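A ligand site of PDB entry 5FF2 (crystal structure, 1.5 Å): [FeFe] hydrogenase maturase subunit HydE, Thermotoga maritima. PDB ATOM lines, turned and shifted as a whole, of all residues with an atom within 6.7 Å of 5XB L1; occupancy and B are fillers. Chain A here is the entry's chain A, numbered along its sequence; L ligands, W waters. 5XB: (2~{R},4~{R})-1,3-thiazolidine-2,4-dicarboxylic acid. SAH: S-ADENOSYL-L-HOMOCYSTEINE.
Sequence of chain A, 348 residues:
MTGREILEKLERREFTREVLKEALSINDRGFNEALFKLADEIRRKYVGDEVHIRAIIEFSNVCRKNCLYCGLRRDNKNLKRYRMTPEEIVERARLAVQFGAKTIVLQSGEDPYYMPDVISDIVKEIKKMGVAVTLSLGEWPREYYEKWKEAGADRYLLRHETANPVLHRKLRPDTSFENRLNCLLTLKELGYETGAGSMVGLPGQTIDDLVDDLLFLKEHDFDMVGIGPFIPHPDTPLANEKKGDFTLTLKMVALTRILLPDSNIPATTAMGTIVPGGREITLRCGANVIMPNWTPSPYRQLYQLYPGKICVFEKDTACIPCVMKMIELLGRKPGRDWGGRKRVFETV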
ATOM      1  N   ILE A  56      18.420  29.289 -15.553  1.00  0.00           N
ATOM      2  CA  ILE A  56      18.543  29.411 -16.980  1.00  0.00           C
ATOM      3  C   ILE A  56      17.251  28.970 -17.692  1.00  0.00           C
ATOM      4  O   ILE A  56      16.761  27.891 -17.435  1.00  0.00           O
ATOM      5  CB  ILE A  56      19.805  28.675 -17.536  1.00  0.00           C
ATOM      6  CG1 ILE A  56      20.005  28.946 -19.025  1.00  0.00           C
ATOM      7  CG2 ILE A  56      19.826  27.198 -17.240  1.00  0.00           C
ATOM      8  CD1 ILE A  56      21.369  28.606 -19.540  1.00  0.00           C
ATOM      9  N   GLU A  58      16.102  28.343 -21.446  1.00  0.00           N
ATOM     10  CA  GLU A  58      16.551  28.101 -22.827  1.00  0.00           C
ATOM     11  C   GLU A  58      15.297  28.278 -23.659  1.00  0.00           C
ATOM     12  O   GLU A  58      14.537  27.366 -23.856  1.00  0.00           O
ATOM     13  CB  GLU A  58      17.165  26.698 -22.917  1.00  0.00           C
ATOM     14  CG  GLU A  58      18.312  26.458 -21.962  1.00  0.00           C
ATOM     15  CD  GLU A  58      18.497  24.962 -21.486  1.00  0.00           C
ATOM     16  OE1 GLU A  58      17.462  24.255 -21.400  1.00  0.00           O
ATOM     17  OE2 GLU A  58      19.588  24.543 -21.159  1.00  0.00           O
ATOM     18  N   VAL A 105      19.063  33.841 -16.413  1.00  0.00           N
ATOM     19  CA  VAL A 105      19.795  33.672 -17.661  1.00  0.00           C
ATOM     20  C   VAL A 105      18.849  33.323 -18.780  1.00  0.00           C
ATOM     21  O   VAL A 105      18.113  32.349 -18.676  1.00  0.00           O
ATOM     22  CB  VAL A 105      20.909  32.590 -17.551  1.00  0.00           C
ATOM     23  CG1 VAL A 105      21.769  32.526 -18.807  1.00  0.00           C
ATOM     24  CG2 VAL A 105      21.822  32.840 -16.329  1.00  0.00           C
ATOM     25  N   GLN A 107      18.977  32.068 -22.510  1.00  0.00           N
ATOM     26  CA  GLN A 107      19.840  31.414 -23.494  1.00  0.00           C
ATOM     27  C   GLN A 107      19.042  30.888 -24.650  1.00  0.00           C
ATOM     28  O   GLN A 107      17.933  30.378 -24.472  1.00  0.00           O
ATOM     29  CB  GLN A 107      20.674  30.322 -22.852  1.00  0.00           C
ATOM     30  CG  GLN A 107      21.790  29.814 -23.810  1.00  0.00           C
ATOM     31  CD  GLN A 107      22.659  28.790 -23.159  1.00  0.00           C
ATOM     32  OE1 GLN A 107      22.275  27.611 -23.128  1.00  0.00           O
ATOM     33  NE2 GLN A 107      23.798  29.168 -22.651  1.00  0.00           N
ATOM     34  N   SER A 136      22.608  35.056 -23.057  1.00  0.00           N
ATOM     35  CA  SER A 136      23.545  34.133 -23.735  1.00  0.00           C
ATOM     36  C   SER A 136      22.918  33.792 -25.078  1.00  0.00           C
ATOM     37  O   SER A 136      22.332  32.746 -25.264  1.00  0.00           O
ATOM     38  CB  SER A 136      23.781  32.932 -22.861  1.00  0.00           C
ATOM     39  OG  SER A 136      24.711  32.019 -23.410  1.00  0.00           O
ATOM     40  N   LEU A 157      27.045  36.006 -21.484  1.00  0.00           N
ATOM     41  CA  LEU A 157      27.893  34.837 -21.620  1.00  0.00           C
ATOM     42  C   LEU A 157      28.166  34.534 -23.068  1.00  0.00           C
ATOM     43  O   LEU A 157      27.208  34.346 -23.843  1.00  0.00           O
ATOM     44  CB  LEU A 157      27.207  33.597 -20.966  1.00  0.00           C
ATOM     45  CG  LEU A 157      26.677  33.774 -19.534  1.00  0.00           C
ATOM     46  CD1 LEU A 157      25.958  32.529 -19.126  1.00  0.00           C
ATOM     47  CD2 LEU A 157      27.787  34.165 -18.588  1.00  0.00           C
ATOM     48  N   ARG A 159      31.017  32.111 -24.602  1.00  0.00           N
ATOM     49  CA  ARG A 159      32.211  31.278 -24.452  1.00  0.00           C
ATOM     50  C   ARG A 159      33.076  31.474 -25.697  1.00  0.00           C
ATOM     51  O   ARG A 159      32.586  31.536 -26.797  1.00  0.00           O
ATOM     52  CB  ARG A 159      31.893  29.814 -24.369  1.00  0.00           C
ATOM     53  CG  ARG A 159      31.334  29.472 -22.976  1.00  0.00           C
ATOM     54  CD  ARG A 159      31.064  27.961 -23.043  1.00  0.00           C
ATOM     55  NE  ARG A 159      30.541  27.482 -21.802  1.00  0.00           N
ATOM     56  CZ  ARG A 159      30.547  26.204 -21.489  1.00  0.00           C
ATOM     57  NH1 ARG A 159      31.015  25.317 -22.369  1.00  0.00           N
ATOM     58  NH2 ARG A 159      30.067  25.850 -20.305  1.00  0.00           N
ATOM     59  N   ALA A 196      33.368  34.238 -20.612  1.00  0.00           N
ATOM     60  CA  ALA A 196      33.989  33.508 -21.721  1.00  0.00           C
ATOM     61  C   ALA A 196      34.141  32.064 -21.274  1.00  0.00           C
ATOM     62  O   ALA A 196      33.335  31.574 -20.467  1.00  0.00           O
ATOM     63  CB  ALA A 196      35.350  34.094 -22.163  1.00  0.00           C
ATOM     64  N   VAL A 225      33.790  32.541 -16.204  1.00  0.00           N
ATOM     65  CA  VAL A 225      34.355  31.553 -17.114  1.00  0.00           C
ATOM     66  C   VAL A 225      33.590  30.221 -17.062  1.00  0.00           C
ATOM     67  O   VAL A 225      33.555  29.581 -15.995  1.00  0.00           O
ATOM     68  CB  VAL A 225      35.838  31.258 -16.809  1.00  0.00           C
ATOM     69  CG1 VAL A 225      36.399  30.299 -17.840  1.00  0.00           C
ATOM     70  CG2 VAL A 225      36.643  32.554 -16.719  1.00  0.00           C
ATOM     71  N   GLY A 226      32.948  29.855 -18.160  1.00  0.00           N
ATOM     72  CA  GLY A 226      32.201  28.625 -18.324  1.00  0.00           C
ATOM     73  C   GLY A 226      33.003  27.572 -19.063  1.00  0.00           C
ATOM     74  O   GLY A 226      33.367  27.773 -20.202  1.00  0.00           O
ATOM     75  N   ILE A 227      33.247  26.448 -18.343  1.00  0.00           N
ATOM     76  CA  ILE A 227      34.092  25.403 -18.916  1.00  0.00           C
ATOM     77  C   ILE A 227      33.352  24.093 -18.758  1.00  0.00           C
ATOM     78  O   ILE A 227      32.802  23.763 -17.660  1.00  0.00           O
ATOM     79  CB  ILE A 227      35.414  25.328 -18.156  1.00  0.00           C
ATOM     80  CG1 ILE A 227      36.268  26.564 -18.472  1.00  0.00           C
ATOM     81  CG2 ILE A 227      36.212  24.040 -18.524  1.00  0.00           C
ATOM     82  CD1 ILE A 227      37.490  26.751 -17.674  1.00  0.00           C
ATOM     83  N   GLY A 228      33.331  23.299 -19.830  1.00  0.00           N
ATOM     84  CA  GLY A 228      32.864  21.968 -19.757  1.00  0.00           C
ATOM     85  C   GLY A 228      33.559  21.106 -20.787  1.00  0.00           C
ATOM     86  O   GLY A 228      34.220  21.590 -21.723  1.00  0.00           O
ATOM     87  N   PRO A 229      33.261  19.780 -20.636  1.00  0.00           N
ATOM     88  CA  PRO A 229      33.797  18.865 -21.655  1.00  0.00           C
ATOM     89  C   PRO A 229      32.965  18.971 -22.950  1.00  0.00           C
ATOM     90  O   PRO A 229      31.820  19.211 -22.918  1.00  0.00           O
ATOM     91  CB  PRO A 229      33.632  17.479 -20.973  1.00  0.00           C
ATOM     92  CG  PRO A 229      32.348  17.627 -20.232  1.00  0.00           C
ATOM     93  CD  PRO A 229      32.467  19.028 -19.611  1.00  0.00           C
ATOM     94  N   PRO A 266      31.048  28.674 -13.039  1.00  0.00           N
ATOM     95  CA  PRO A 266      30.048  27.638 -12.798  1.00  0.00           C
ATOM     96  C   PRO A 266      30.552  26.234 -12.794  1.00  0.00           C
ATOM     97  O   PRO A 266      31.559  25.933 -13.487  1.00  0.00           O
ATOM     98  CB  PRO A 266      29.084  27.821 -13.950  1.00  0.00           C
ATOM     99  CG  PRO A 266      29.942  28.415 -15.028  1.00  0.00           C
ATOM    100  CD  PRO A 266      30.798  29.381 -14.304  1.00  0.00           C
ATOM    101  N   ALA A 267      29.857  25.390 -12.059  1.00  0.00           N
ATOM    102  CA  ALA A 267      29.898  23.939 -12.182  1.00  0.00           C
ATOM    103  C   ALA A 267      28.872  23.602 -13.232  1.00  0.00           C
ATOM    104  O   ALA A 267      27.665  23.572 -12.943  1.00  0.00           O
ATOM    105  CB  ALA A 267      29.614  23.255 -10.846  1.00  0.00           C
ATOM    106  N   THR A 268      29.302  23.365 -14.467  1.00  0.00           N
ATOM    107  CA  THR A 268      28.375  23.304 -15.595  1.00  0.00           C
ATOM    108  C   THR A 268      27.601  22.022 -15.655  1.00  0.00           C
ATOM    109  O   THR A 268      28.044  20.954 -15.177  1.00  0.00           O
ATOM    110  CB  THR A 268      29.144  23.601 -16.918  1.00  0.00           C
ATOM    111  OG1 THR A 268      30.118  22.569 -17.120  1.00  0.00           O
ATOM    112  CG2 THR A 268      29.803  24.944 -16.965  1.00  0.00           C
ATOM    113  N   THR A 269      26.435  22.085 -16.276  1.00  0.00           N
ATOM    114  CA  THR A 269      25.639  20.910 -16.559  1.00  0.00           C
ATOM    115  C   THR A 269      26.400  19.851 -17.346  1.00  0.00           C
ATOM    116  O   THR A 269      26.215  18.658 -17.020  1.00  0.00           O
ATOM    117  CB  THR A 269      24.301  21.282 -17.187  1.00  0.00           C
ATOM    118  OG1 THR A 269      23.592  22.126 -16.288  1.00  0.00           O
ATOM    119  CG2 THR A 269      23.458  20.013 -17.450  1.00  0.00           C
ATOM    120  N   ALA A 270      27.260  20.232 -18.263  1.00  0.00           N
ATOM    121  CA  ALA A 270      28.028  19.262 -19.003  1.00  0.00           C
ATOM    122  C   ALA A 270      28.918  18.422 -18.044  1.00  0.00           C
ATOM    123  O   ALA A 270      29.096  17.209 -18.221  1.00  0.00           O
ATOM    124  CB  ALA A 270      28.825  19.918 -20.111  1.00  0.00           C
ATOM    125  N   MET A 271      29.466  19.051 -17.028  1.00  0.00           N
ATOM    126  CA  MET A 271      30.288  18.335 -16.032  1.00  0.00           C
ATOM    127  C   MET A 271      29.422  17.292 -15.290  1.00  0.00           C
ATOM    128  O   MET A 271      29.905  16.207 -15.006  1.00  0.00           O
ATOM    129  CB  MET A 271      30.911  19.296 -15.020  1.00  0.00           C
ATOM    130  CG  MET A 271      32.108  20.063 -15.677  1.00  0.00           C
ATOM    131  SD  MET A 271      33.463  18.999 -16.076  1.00  0.00           S
ATOM    132  CE  MET A 271      34.637  19.290 -14.719  1.00  0.00           C
ATOM    133  N   THR A 273      26.816  15.821 -16.551  1.00  0.00           N
ATOM    134  CA  THR A 273      26.366  14.886 -17.598  1.00  0.00           C
ATOM    135  C   THR A 273      27.410  13.795 -17.827  1.00  0.00           C
ATOM    136  O   THR A 273      27.019  12.634 -17.958  1.00  0.00           O
ATOM    137  CB  THR A 273      25.989  15.671 -18.872  1.00  0.00           C
ATOM    138  OG1 THR A 273      24.938  16.588 -18.549  1.00  0.00           O
ATOM    139  CG2 THR A 273      25.484  14.713 -19.960  1.00  0.00           C
ATOM    140  N   MET A 291      23.900  26.675 -12.301  1.00  0.00           N
ATOM    141  CA  MET A 291      22.852  27.172 -13.192  1.00  0.00           C
ATOM    142  C   MET A 291      21.674  26.124 -13.411  1.00  0.00           C
ATOM    143  O   MET A 291      21.647  25.338 -14.408  1.00  0.00           O
ATOM    144  CB  MET A 291      23.515  27.577 -14.525  1.00  0.00           C
ATOM    145  CG  MET A 291      24.687  28.569 -14.317  1.00  0.00           C
ATOM    146  SD  MET A 291      25.805  28.812 -15.768  1.00  0.00           S
ATOM    147  CE  MET A 291      24.480  29.836 -16.297  1.00  0.00           C
ATOM    148  N   LEU A 305      22.059  20.590 -26.820  1.00  0.00           N
ATOM    149  CA  LEU A 305      23.356  20.967 -27.335  1.00  0.00           C
ATOM    150  C   LEU A 305      24.145  19.688 -27.443  1.00  0.00           C
ATOM    151  O   LEU A 305      24.826  19.490 -28.400  1.00  0.00           O
ATOM    152  CB  LEU A 305      24.001  21.948 -26.334  1.00  0.00           C
ATOM    153  CG  LEU A 305      23.244  23.220 -26.021  1.00  0.00           C
ATOM    154  CD1 LEU A 305      24.015  23.940 -24.885  1.00  0.00           C
ATOM    155  CD2 LEU A 305      23.152  24.077 -27.238  1.00  0.00           C
ATOM    156  N   TYR A 306      24.047  18.850 -26.441  1.00  0.00           N
ATOM    157  CA  TYR A 306      24.628  17.554 -26.342  1.00  0.00           C
ATOM    158  C   TYR A 306      23.602  16.607 -25.751  1.00  0.00           C
ATOM    159  O   TYR A 306      22.628  17.094 -25.077  1.00  0.00           O
ATOM    160  CB  TYR A 306      25.899  17.556 -25.522  1.00  0.00           C
ATOM    161  CG  TYR A 306      25.757  18.201 -24.153  1.00  0.00           C
ATOM    162  CD1 TYR A 306      25.309  17.470 -23.084  1.00  0.00           C
ATOM    163  CD2 TYR A 306      26.046  19.517 -23.978  1.00  0.00           C
ATOM    164  CE1 TYR A 306      25.151  18.022 -21.866  1.00  0.00           C
ATOM    165  CE2 TYR A 306      25.894  20.125 -22.749  1.00  0.00           C
ATOM    166  CZ  TYR A 306      25.458  19.366 -21.680  1.00  0.00           C
ATOM    167  OH  TYR A 306      25.241  19.926 -20.485  1.00  0.00           O
HETATM  168  C2  5XB L   1      26.534  27.065 -19.498  1.00  0.00           C
HETATM  169  C4  5XB L   1      25.878  24.789 -20.135  1.00  0.00           C
HETATM  170  C5  5XB L   1      26.195  25.270 -21.559  1.00  0.00           C
HETATM  171  S1  5XB L   1      26.484  27.049 -21.304  1.00  0.00           S
HETATM  172  O41 5XB L   1      25.199  22.550 -20.489  1.00  0.00           O
HETATM  173  C4A 5XB L   1      26.077  23.264 -20.035  1.00  0.00           C
HETATM  174  O42 5XB L   1      27.064  22.847 -19.489  1.00  0.00           O
HETATM  175  C2A 5XB L   1      27.675  27.961 -18.963  1.00  0.00           C
HETATM  176  O21 5XB L   1      27.472  29.152 -18.838  1.00  0.00           O
HETATM  177  O22 5XB L   1      28.718  27.478 -18.674  1.00  0.00           O
HETATM  178  N3  5XB L   1      26.667  25.622 -19.259  1.00  0.00           N
HETATM  179  N   SAH L   2      24.181  30.112 -29.208  1.00  0.00           N
HETATM  180  CA  SAH L   2      24.880  30.620 -28.056  1.00  0.00           C
HETATM  181  CB  SAH L   2      24.420  29.961 -26.811  1.00  0.00           C
HETATM  182  CG  SAH L   2      23.905  28.536 -26.748  1.00  0.00           C
HETATM  183  SD  SAH L   2      25.260  27.399 -26.857  1.00  0.00           S
HETATM  184  C   SAH L   2      26.329  30.511 -28.261  1.00  0.00           C
HETATM  185  O   SAH L   2      26.988  31.237 -27.493  1.00  0.00           O
HETATM  186  OXT SAH L   2      26.811  29.727 -29.119  1.00  0.00           O
HETATM  187  C5' SAH L   2      25.963  27.374 -25.216  1.00  0.00           C
HETATM  188  C4' SAH L   2      27.295  26.671 -25.136  1.00  0.00           C
HETATM  189  O4' SAH L   2      27.116  25.230 -25.139  1.00  0.00           O
HETATM  190  C3' SAH L   2      28.369  26.857 -26.197  1.00  0.00           C
HETATM  191  O3' SAH L   2      29.099  28.059 -25.905  1.00  0.00           O
HETATM  192  C2' SAH L   2      29.206  25.578 -26.107  1.00  0.00           C
HETATM  193  O2' SAH L   2      30.475  25.739 -25.441  1.00  0.00           O
HETATM  194  C1' SAH L   2      28.292  24.558 -25.427  1.00  0.00           C
HETATM  195  N9  SAH L   2      28.063  23.402 -26.240  1.00  0.00           N
HETATM  196  C8  SAH L   2      27.462  23.331 -27.484  1.00  0.00           C
HETATM  197  N7  SAH L   2      27.539  22.085 -27.985  1.00  0.00           N
HETATM  198  C5  SAH L   2      28.221  21.355 -27.087  1.00  0.00           C
HETATM  199  C6  SAH L   2      28.582  19.971 -26.992  1.00  0.00           C
HETATM  200  N6  SAH L   2      28.350  19.102 -27.977  1.00  0.00           N
HETATM  201  N1  SAH L   2      29.240  19.566 -25.899  1.00  0.00           N
HETATM  202  C2  SAH L   2      29.459  20.430 -24.866  1.00  0.00           C
HETATM  203  N3  SAH L   2      29.129  21.677 -24.907  1.00  0.00           N
HETATM  204  C4  SAH L   2      28.504  22.202 -25.945  1.00  0.00           C
HETATM  205  O   HOH W   1      29.452  30.924 -17.323  1.00  0.00           O
HETATM  206  O   HOH W   2      29.717  23.166 -20.108  1.00  0.00           O
HETATM  207  O   HOH W   3      25.445  24.831 -16.655  1.00  0.00           O
HETATM  208  O   HOH W   4      22.862  22.935 -21.607  1.00  0.00           O
HETATM  209  O   HOH W   5      28.921  30.128 -20.757  1.00  0.00           O
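An oxygen (O22) of 5XB L1 lies within salt-bridge range of the guanidinium group (NH2) of Arg 159 (2.7 Å). The backbone NH (N) of Thr 269 sits at hydrogen-bond distance from an oxygen (O42) of 5XB L1 (3.4 Å). NH1 of Arg 159 lies within hydrogen-bond range of O2' of SAH L2, at 3.1 Å. OH of Tyr 306 is in hydrogen-bond range of O41 of 5XB L1 (2.6 Å). A sulfur (S1) of 5XB L1 sits close to the side-chain amide nitrogen (NE2) of Gln 107. The backbone NH (N) of Ala 270 is in hydrogen-bond range of an oxygen (O42) of 5XB L1 (2.9 Å).
OG of Ser 136 is in hydrogen-bond range of O of Leu 157 (3.4 Å). The backbone carbonyl oxygen of Gly 226 sits at hydrogen-bond distance from the guanidinium group of Arg 159 (3.3 Å). The side-chain amide nitrogen of Gln 107 lies within hydrogen-bond range of the side-chain hydroxyl of Ser 136 (3.1 Å). The backbone NH (N) of Gly 226 sits at hydrogen-bond distance from the backbone carbonyl oxygen (O) of Ala 196. The backbone carbonyl oxygen (O) of Thr 269 sits at hydrogen-bond distance from the side-chain hydroxyl (OG1) of Thr 273 (2.9 Å). The backbone carbonyl oxygen of Ile 227 is in hydrogen-bond range of the side-chain hydroxyl of Thr 268, 3.0 Å away. The side-chain hydroxyl (OH) of Tyr 306 is in hydrogen-bond range of the backbone NH (N) of Ala 270 (3.0 Å).
An oxygen (O21) of 5XB L1 lies close to the side-chain sulfur (SD) of Met 291 (3.5 Å). Residues that only touch 5XB L1: Leu 157 (3.7 Å), Gly 226 (3.7 Å), Pro 266 (3.96 Å) and Thr 268 (3.2 Å). Hydrophobic or aromatic side chains that line 5XB L1: Leu 157, Pro 266, Ala 270, Met 291 and Tyr 306. Within 4 Å of 5XB L1: Gln 107, Leu 157, Arg 159, Gly 226, Pro 266, Thr 268, Thr 269, Ala 270, Met 291 and Tyr 306.
Water W5 bridges O21 of 5XB L1 (2.6 Å) and NE of Arg 159 (3.3 Å). Water W2 lies within hydrogen-bond range of NH2 of Arg 159 (2.7 Å), O42 of 5XB L1 (2.7 Å) and OG1 of Thr 268 (3.1 Å). Water W3 lies within hydrogen-bond range of the backbone NH (N) of Thr 269 (2.9 Å) and a nitrogen (N3) of 5XB L1 (3.0 Å).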
